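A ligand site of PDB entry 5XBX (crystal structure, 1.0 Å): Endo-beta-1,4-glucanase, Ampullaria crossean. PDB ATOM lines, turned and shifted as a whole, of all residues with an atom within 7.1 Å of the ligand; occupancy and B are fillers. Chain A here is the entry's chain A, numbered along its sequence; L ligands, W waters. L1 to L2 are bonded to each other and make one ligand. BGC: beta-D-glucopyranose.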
ATOM      1  N   THR A  27     -25.740 -18.168  11.460  1.00  0.00           N
ATOM      2  CA  THR A  27     -26.105 -18.690  12.758  1.00  0.00           C
ATOM      3  C   THR A  27     -25.945 -20.197  12.780  1.00  0.00           C
ATOM      4  O   THR A  27     -26.069 -20.869  11.751  1.00  0.00           O
ATOM      5  CB  THR A  27     -27.522 -18.298  13.178  1.00  0.00           C
ATOM      6  OG1 THR A  27     -28.502 -19.054  12.460  1.00  0.00           O
ATOM      7  CG2 THR A  27     -27.827 -16.838  13.070  1.00  0.00           C
ATOM      8  N   THR A  28     -25.701 -20.716  13.990  1.00  0.00           N
ATOM      9  CA  THR A  28     -25.755 -22.138  14.288  1.00  0.00           C
ATOM     10  C   THR A  28     -26.447 -22.286  15.637  1.00  0.00           C
ATOM     11  O   THR A  28     -26.882 -21.296  16.243  1.00  0.00           O
ATOM     12  CB  THR A  28     -24.365 -22.784  14.273  1.00  0.00           C
ATOM     13  OG1 THR A  28     -23.450 -22.038  15.092  1.00  0.00           O
ATOM     14  CG2 THR A  28     -23.763 -22.915  12.868  1.00  0.00           C
ATOM     15  N   ARG A  29     -26.547 -23.529  16.123  1.00  0.00           N
ATOM     16  CA  ARG A  29     -27.079 -23.802  17.449  1.00  0.00           C
ATOM     17  C   ARG A  29     -26.067 -24.658  18.188  1.00  0.00           C
ATOM     18  O   ARG A  29     -25.323 -25.419  17.578  1.00  0.00           O
ATOM     19  CB  ARG A  29     -28.447 -24.467  17.353  1.00  0.00           C
ATOM     20  CG  ARG A  29     -28.469 -25.764  16.554  1.00  0.00           C
ATOM     21  CD  ARG A  29     -29.915 -26.206  16.163  1.00  0.00           C
ATOM     22  NE  ARG A  29     -29.909 -27.397  15.309  1.00  0.00           N
ATOM     23  CZ  ARG A  29     -29.750 -27.419  13.982  1.00  0.00           C
ATOM     24  NH1 ARG A  29     -29.579 -26.304  13.271  1.00  0.00           N
ATOM     25  NH2 ARG A  29     -29.771 -28.587  13.346  1.00  0.00           N
ATOM     26  N   TYR A  30     -26.047 -24.515  19.519  1.00  0.00           N
ATOM     27  CA  TYR A  30     -25.110 -25.294  20.304  1.00  0.00           C
ATOM     28  C   TYR A  30     -25.727 -25.663  21.637  1.00  0.00           C
ATOM     29  O   TYR A  30     -26.632 -25.000  22.138  1.00  0.00           O
ATOM     30  CB  TYR A  30     -23.816 -24.536  20.555  1.00  0.00           C
ATOM     31  CG  TYR A  30     -23.816 -23.465  21.642  1.00  0.00           C
ATOM     32  CD1 TYR A  30     -24.346 -22.206  21.422  1.00  0.00           C
ATOM     33  CD2 TYR A  30     -23.236 -23.722  22.880  1.00  0.00           C
ATOM     34  CE1 TYR A  30     -24.283 -21.203  22.401  1.00  0.00           C
ATOM     35  CE2 TYR A  30     -23.176 -22.735  23.866  1.00  0.00           C
ATOM     36  CZ  TYR A  30     -23.696 -21.479  23.626  1.00  0.00           C
ATOM     37  OH  TYR A  30     -23.605 -20.519  24.621  1.00  0.00           O
ATOM     38  N   VAL A  31     -25.192 -26.729  22.212  1.00  0.00           N
ATOM     39  CA  VAL A  31     -25.493 -27.127  23.579  1.00  0.00           C
ATOM     40  C   VAL A  31     -24.156 -27.534  24.179  1.00  0.00           C
ATOM     41  O   VAL A  31     -23.363 -28.225  23.530  1.00  0.00           O
ATOM     42  CB  VAL A  31     -26.567 -28.250  23.614  1.00  0.00           C
ATOM     43  CG1 VAL A  31     -27.906 -27.817  22.999  1.00  0.00           C
ATOM     44  CG2 VAL A  31     -26.069 -29.478  22.913  1.00  0.00           C
ATOM     45  N   ASP A  32     -23.864 -27.093  25.411  1.00  0.00           N
ATOM     46  CA  ASP A  32     -22.664 -27.618  26.067  1.00  0.00           C
ATOM     47  C   ASP A  32     -22.738 -27.581  27.577  1.00  0.00           C
ATOM     48  O   ASP A  32     -21.845 -28.152  28.235  1.00  0.00           O
ATOM     49  CB  ASP A  32     -21.361 -26.977  25.546  1.00  0.00           C
ATOM     50  CG  ASP A  32     -21.233 -25.498  25.874  1.00  0.00           C
ATOM     51  OD1 ASP A  32     -21.912 -24.997  26.789  1.00  0.00           O
ATOM     52  OD2 ASP A  32     -20.428 -24.836  25.175  1.00  0.00           O
ATOM     53  N   ALA A  59     -23.588 -17.120  21.801  1.00  0.00           N
ATOM     54  CA  ALA A  59     -22.145 -17.072  21.793  1.00  0.00           C
ATOM     55  C   ALA A  59     -21.719 -16.557  20.410  1.00  0.00           C
ATOM     56  O   ALA A  59     -21.672 -17.340  19.445  1.00  0.00           O
ATOM     57  CB  ALA A  59     -21.569 -18.463  22.032  1.00  0.00           C
ATOM     58  N   VAL A  91     -26.886 -21.517   4.272  1.00  0.00           N
ATOM     59  CA  VAL A  91     -25.741 -22.054   3.548  1.00  0.00           C
ATOM     60  C   VAL A  91     -26.143 -23.414   3.006  1.00  0.00           C
ATOM     61  O   VAL A  91     -26.587 -24.279   3.780  1.00  0.00           O
ATOM     62  CB  VAL A  91     -24.500 -22.163   4.437  1.00  0.00           C
ATOM     63  CG1 VAL A  91     -23.375 -22.859   3.716  1.00  0.00           C
ATOM     64  CG2 VAL A  91     -24.088 -20.788   4.911  1.00  0.00           C
ATOM     65  N   GLY A  93     -26.673 -27.044   2.240  1.00  0.00           N
ATOM     66  CA  GLY A  93     -26.193 -28.228   2.904  1.00  0.00           C
ATOM     67  C   GLY A  93     -25.893 -28.049   4.381  1.00  0.00           C
ATOM     68  O   GLY A  93     -25.526 -29.028   5.051  1.00  0.00           O
ATOM     69  N   LYS A  94     -26.055 -26.841   4.913  1.00  0.00           N
ATOM     70  CA  LYS A  94     -25.711 -26.512   6.295  1.00  0.00           C
ATOM     71  C   LYS A  94     -26.788 -25.639   6.929  1.00  0.00           C
ATOM     72  O   LYS A  94     -26.497 -24.714   7.688  1.00  0.00           O
ATOM     73  CB  LYS A  94     -24.342 -25.859   6.379  1.00  0.00           C
ATOM     74  CG  LYS A  94     -23.311 -26.734   5.769  1.00  0.00           C
ATOM     75  CD  LYS A  94     -21.963 -26.495   6.223  1.00  0.00           C
ATOM     76  CE  LYS A  94     -21.083 -27.596   5.736  1.00  0.00           C
ATOM     77  NZ  LYS A  94     -19.925 -26.961   5.108  1.00  0.00           N
ATOM     78  N   GLY A  95     -28.040 -25.941   6.610  1.00  0.00           N
ATOM     79  CA  GLY A  95     -29.150 -25.202   7.147  1.00  0.00           C
ATOM     80  C   GLY A  95     -30.344 -25.378   6.243  1.00  0.00           C
ATOM     81  O   GLY A  95     -30.349 -26.224   5.350  1.00  0.00           O
ATOM     82  N   CYS A 112     -17.915 -17.782  20.942  1.00  0.00           N
ATOM     83  CA  CYS A 112     -17.577 -18.833  19.985  1.00  0.00           C
ATOM     84  C   CYS A 112     -16.139 -18.594  19.542  1.00  0.00           C
ATOM     85  O   CYS A 112     -15.898 -17.721  18.686  1.00  0.00           O
ATOM     86  CB  CYS A 112     -18.536 -18.789  18.805  1.00  0.00           C
ATOM     87  SG  CYS A 112     -18.226 -20.084  17.562  1.00  0.00           S
ATOM     88  N   PRO A 113     -15.159 -19.270  20.150  1.00  0.00           N
ATOM     89  CA  PRO A 113     -13.758 -18.958  19.841  1.00  0.00           C
ATOM     90  C   PRO A 113     -13.403 -19.396  18.442  1.00  0.00           C
ATOM     91  O   PRO A 113     -13.927 -20.379  17.923  1.00  0.00           O
ATOM     92  CB  PRO A 113     -12.981 -19.786  20.860  1.00  0.00           C
ATOM     93  CG  PRO A 113     -13.938 -20.887  21.281  1.00  0.00           C
ATOM     94  CD  PRO A 113     -15.300 -20.311  21.182  1.00  0.00           C
ATOM     95  N   GLY A 116     -11.208 -24.188  17.304  1.00  0.00           N
ATOM     96  CA  GLY A 116     -12.224 -25.221  17.307  1.00  0.00           C
ATOM     97  C   GLY A 116     -13.490 -24.859  16.563  1.00  0.00           C
ATOM     98  O   GLY A 116     -14.393 -25.700  16.481  1.00  0.00           O
ATOM     99  N   ASN A 117     -13.585 -23.652  15.997  1.00  0.00           N
ATOM    100  CA  ASN A 117     -14.766 -23.234  15.259  1.00  0.00           C
ATOM    101  C   ASN A 117     -14.371 -22.471  14.009  1.00  0.00           C
ATOM    102  O   ASN A 117     -14.851 -21.363  13.763  1.00  0.00           O
ATOM    103  CB  ASN A 117     -15.711 -22.389  16.114  1.00  0.00           C
ATOM    104  CG  ASN A 117     -16.180 -23.122  17.359  1.00  0.00           C
ATOM    105  OD1 ASN A 117     -17.094 -23.950  17.320  1.00  0.00           O
ATOM    106  ND2 ASN A 117     -15.511 -22.828  18.485  1.00  0.00           N
ATOM    107  N   GLU A 118     -13.507 -23.061  13.186  1.00  0.00           N
ATOM    108  CA  GLU A 118     -12.964 -22.316  12.049  1.00  0.00           C
ATOM    109  C   GLU A 118     -14.060 -21.935  11.067  1.00  0.00           C
ATOM    110  O   GLU A 118     -14.111 -20.780  10.610  1.00  0.00           O
ATOM    111  CB  GLU A 118     -11.885 -23.129  11.346  1.00  0.00           C
ATOM    112  CG  GLU A 118     -11.430 -22.539   9.974  1.00  0.00           C
ATOM    113  CD  GLU A 118     -10.782 -21.141  10.045  1.00  0.00           C
ATOM    114  OE1 GLU A 118     -10.607 -20.534   8.954  1.00  0.00           O
ATOM    115  OE2 GLU A 118     -10.423 -20.657  11.133  1.00  0.00           O
ATOM    116  N   GLU A 119     -14.906 -22.884  10.680  1.00  0.00           N
ATOM    117  CA  GLU A 119     -15.824 -22.670   9.565  1.00  0.00           C
ATOM    118  C   GLU A 119     -16.716 -21.465   9.804  1.00  0.00           C
ATOM    119  O   GLU A 119     -16.912 -20.636   8.899  1.00  0.00           O
ATOM    120  CB  GLU A 119     -16.680 -23.932   9.397  1.00  0.00           C
ATOM    121  CG  GLU A 119     -17.829 -23.711   8.403  1.00  0.00           C
ATOM    122  CD  GLU A 119     -18.572 -24.979   8.034  1.00  0.00           C
ATOM    123  OE1 GLU A 119     -19.397 -24.913   7.108  1.00  0.00           O
ATOM    124  OE2 GLU A 119     -18.329 -26.043   8.645  1.00  0.00           O
ATOM    125  N   TRP A 120     -17.308 -21.372  10.995  1.00  0.00           N
ATOM    126  CA  TRP A 120     -18.288 -20.337  11.307  1.00  0.00           C
ATOM    127  C   TRP A 120     -17.712 -19.151  12.056  1.00  0.00           C
ATOM    128  O   TRP A 120     -18.142 -18.017  11.834  1.00  0.00           O
ATOM    129  CB  TRP A 120     -19.458 -20.932  12.108  1.00  0.00           C
ATOM    130  CG  TRP A 120     -20.174 -22.028  11.367  1.00  0.00           C
ATOM    131  CD1 TRP A 120     -20.090 -23.372  11.621  1.00  0.00           C
ATOM    132  CD2 TRP A 120     -21.120 -21.891  10.282  1.00  0.00           C
ATOM    133  NE1 TRP A 120     -20.910 -24.076  10.774  1.00  0.00           N
ATOM    134  CE2 TRP A 120     -21.557 -23.197   9.954  1.00  0.00           C
ATOM    135  CE3 TRP A 120     -21.649 -20.796   9.580  1.00  0.00           C
ATOM    136  CZ2 TRP A 120     -22.489 -23.434   8.964  1.00  0.00           C
ATOM    137  CZ3 TRP A 120     -22.585 -21.035   8.569  1.00  0.00           C
ATOM    138  CH2 TRP A 120     -22.993 -22.358   8.273  1.00  0.00           C
ATOM    139  N   CYS A 121     -16.797 -19.403  12.996  1.00  0.00           N
ATOM    140  CA  CYS A 121     -16.306 -18.350  13.878  1.00  0.00           C
ATOM    141  C   CYS A 121     -14.895 -17.887  13.574  1.00  0.00           C
ATOM    142  O   CYS A 121     -14.401 -16.954  14.222  1.00  0.00           O
ATOM    143  CB  CYS A 121     -16.439 -18.787  15.346  1.00  0.00           C
ATOM    144  SG  CYS A 121     -18.174 -19.122  15.721  1.00  0.00           S
ATOM    145  N   HIS A 140     -20.810 -14.218  13.309  1.00  0.00           N
ATOM    146  CA  HIS A 140     -21.546 -15.449  13.458  1.00  0.00           C
ATOM    147  C   HIS A 140     -22.166 -15.475  14.856  1.00  0.00           C
ATOM    148  O   HIS A 140     -21.508 -15.085  15.825  1.00  0.00           O
ATOM    149  CB  HIS A 140     -20.616 -16.644  13.320  1.00  0.00           C
ATOM    150  CG  HIS A 140     -21.351 -17.928  13.353  1.00  0.00           C
ATOM    151  ND1 HIS A 140     -22.049 -18.379  12.251  1.00  0.00           N
ATOM    152  CD2 HIS A 140     -21.583 -18.796  14.368  1.00  0.00           C
ATOM    153  CE1 HIS A 140     -22.654 -19.494  12.601  1.00  0.00           C
ATOM    154  NE2 HIS A 140     -22.389 -19.780  13.865  1.00  0.00           N
ATOM    155  N   ASP A 142     -23.762 -18.157  17.459  1.00  0.00           N
ATOM    156  CA  ASP A 142     -24.083 -19.524  17.871  1.00  0.00           C
ATOM    157  C   ASP A 142     -25.172 -19.413  18.925  1.00  0.00           C
ATOM    158  O   ASP A 142     -25.011 -18.708  19.926  1.00  0.00           O
ATOM    159  CB  ASP A 142     -22.827 -20.212  18.396  1.00  0.00           C
ATOM    160  CG  ASP A 142     -22.861 -21.726  18.303  1.00  0.00           C
ATOM    161  OD1 ASP A 142     -23.783 -22.289  17.699  1.00  0.00           O
ATOM    162  OD2 ASP A 142     -21.897 -22.306  18.847  1.00  0.00           O
ATOM    163  N   ASP A 156     -33.006 -23.561  11.446  1.00  0.00           N
ATOM    164  CA  ASP A 156     -31.934 -24.475  11.083  1.00  0.00           C
ATOM    165  C   ASP A 156     -30.839 -23.643  10.416  1.00  0.00           C
ATOM    166  O   ASP A 156     -30.820 -23.451   9.197  1.00  0.00           O
ATOM    167  CB  ASP A 156     -32.429 -25.553  10.153  1.00  0.00           C
ATOM    168  CG  ASP A 156     -31.357 -26.546   9.782  1.00  0.00           C
ATOM    169  OD1 ASP A 156     -30.266 -26.545  10.382  1.00  0.00           O
ATOM    170  OD2 ASP A 156     -31.629 -27.351   8.876  1.00  0.00           O
ATOM    171  N   ASN A 157     -29.952 -23.116  11.245  1.00  0.00           N
ATOM    172  CA  ASN A 157     -28.850 -22.259  10.813  1.00  0.00           C
ATOM    173  C   ASN A 157     -29.269 -21.176   9.814  1.00  0.00           C
ATOM    174  O   ASN A 157     -28.600 -20.987   8.792  1.00  0.00           O
ATOM    175  CB  ASN A 157     -27.717 -23.092  10.238  1.00  0.00           C
ATOM    176  CG  ASN A 157     -27.206 -24.156  11.151  1.00  0.00           C
ATOM    177  OD1 ASN A 157     -27.475 -24.174  12.349  1.00  0.00           O
ATOM    178  ND2 ASN A 157     -26.413 -25.050  10.592  1.00  0.00           N
HETATM  179  C2  BGC L   1     -23.410 -27.349  10.665  1.00  0.00           C
HETATM  180  C3  BGC L   1     -22.660 -27.457  11.953  1.00  0.00           C
HETATM  181  C4  BGC L   1     -23.373 -26.907  13.164  1.00  0.00           C
HETATM  182  C5  BGC L   1     -24.797 -27.523  13.163  1.00  0.00           C
HETATM  183  C6  BGC L   1     -25.734 -26.975  14.223  1.00  0.00           C
HETATM  184  C1  BGC L   1     -24.786 -27.973  10.773  1.00  0.00           C
HETATM  185  O1  BGC L   1     -25.466 -27.781   9.629  1.00  0.00           O
HETATM  186  O2  BGC L   1     -22.703 -28.008   9.605  1.00  0.00           O
HETATM  187  O3  BGC L   1     -21.392 -26.769  11.738  1.00  0.00           O
HETATM  188  O4  BGC L   1     -22.664 -27.287  14.353  1.00  0.00           O
HETATM  189  O5  BGC L   1     -25.468 -27.285  11.885  1.00  0.00           O
HETATM  190  O6  BGC L   1     -25.877 -25.589  14.124  1.00  0.00           O
HETATM  191  C2  BGC L   2     -22.295 -27.109  16.608  1.00  0.00           C
HETATM  192  C3  BGC L   2     -21.848 -26.189  17.702  1.00  0.00           C
HETATM  193  C4  BGC L   2     -20.732 -25.258  17.289  1.00  0.00           C
HETATM  194  C5  BGC L   2     -21.124 -24.479  16.021  1.00  0.00           C
HETATM  195  C6  BGC L   2     -20.067 -23.535  15.517  1.00  0.00           C
HETATM  196  C1  BGC L   2     -22.579 -26.356  15.320  1.00  0.00           C
HETATM  197  O2  BGC L   2     -23.468 -27.814  17.011  1.00  0.00           O
HETATM  198  O3  BGC L   2     -21.435 -27.015  18.819  1.00  0.00           O
HETATM  199  O4  BGC L   2     -20.445 -24.349  18.335  1.00  0.00           O
HETATM  200  O5  BGC L   2     -21.448 -25.457  14.974  1.00  0.00           O
HETATM  201  O6  BGC L   2     -18.828 -24.126  15.232  1.00  0.00           O
HETATM  202  O   HOH W   1     -17.093 -23.511  13.053  1.00  0.00           O
HETATM  203  O   HOH W   2     -21.028 -27.064  21.340  1.00  0.00           O
HETATM  204  O   HOH W   3     -23.560 -28.309  20.225  1.00  0.00           O
HETATM  205  O   HOH W   4     -28.229 -28.308   9.942  1.00  0.00           O
HETATM  206  O   HOH W   5     -20.268 -27.884   8.746  1.00  0.00           O
HETATM  207  O   HOH W   6     -18.992 -26.798  13.980  1.00  0.00           O
HETATM  208  O   HOH W   7     -18.225 -25.026  19.772  1.00  0.00           O
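OD1 of Asp 142 sits close to N of Arg 29 (3.4 Å). The side-chain carboxylate (OD1) of Asp 142 is in hydrogen-bond range of the side-chain hydroxyl (OG1) of Thr 28 (2.6 Å). The backbone carbonyl oxygen (O) of Asp 142 sits at hydrogen-bond distance from the backbone NH (N) of Ala 59. The side-chain amide nitrogen (ND2) of Asn 117 lies within hydrogen-bond range of the backbone carbonyl oxygen (O) of Pro 113, at 3.0 Å. The side-chain amide oxygen of Asn 157 lies within hydrogen-bond range of the guanidinium group of Arg 29 (3.1 Å). The guanidinium group (NH1) of Arg 29 is in salt-bridge range of the side-chain carboxylate (OD1) of Asp 156, 3.0 Å away. The side-chain hydroxyl (OG1) of Thr 28 sits at hydrogen-bond distance from a ring nitrogen (NE2) of His 140 (2.8 Å). OE1 of Glu 119 is in salt-bridge range of NZ of Lys 94 (2.9 Å).
The side-chain carboxylate (OD2) of Asp 142 is in hydrogen-bond range of an oxygen (O4) of BGC L2 (2.6 Å). The side-chain amide oxygen of Asn 117 is in hydrogen-bond range of an oxygen (O6) of BGC L2 (2.7 Å). ND2 of Asn 157 sits at hydrogen-bond distance from O5 of BGC L1 (2.7 Å). O3 of BGC L1 lies within hydrogen-bond range of NE1 of Trp 120 (2.9 Å). An oxygen (O6) of BGC L1 is in hydrogen-bond range of the backbone NH (N) of Arg 29, at 2.9 Å. O2 of BGC L2 lies within hydrogen-bond range of O of Arg 29 (3.1 Å).
CB of Thr 28 touches O6 of BGC L1 (3.2 Å). Tyr 30 touches the ligand. CA of Lys 94 touches O1 of BGC L1, 3.6 Å away. Hydrophobic or aromatic side chains that line the ligand: Tyr 30 and Trp 120.
Water W2 bridges an oxygen (O3) of BGC L2 and the backbone carbonyl oxygen (O) of Val 31. Water W5 bridges an oxygen (O2) of BGC L1 (2.6 Å) and the side-chain carboxylate of Glu 119 (2.7 Å). Water W7 lies within hydrogen-bond range of O4 of BGC L2 (2.7 Å) and OD1 of Asn 117 (2.9 Å). Water W4 lies within hydrogen-bond range of the side-chain carboxylate of Asp 156 and an oxygen (O1) of BGC L1. Water W1 lies within hydrogen-bond range of O6 of BGC L2, N of Trp 120, O of Asn 117 and N of Glu 119. Water W3 lies within hydrogen-bond range of O3 of BGC L2 (2.9 Å) and N of Val 31 (3.0 Å).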
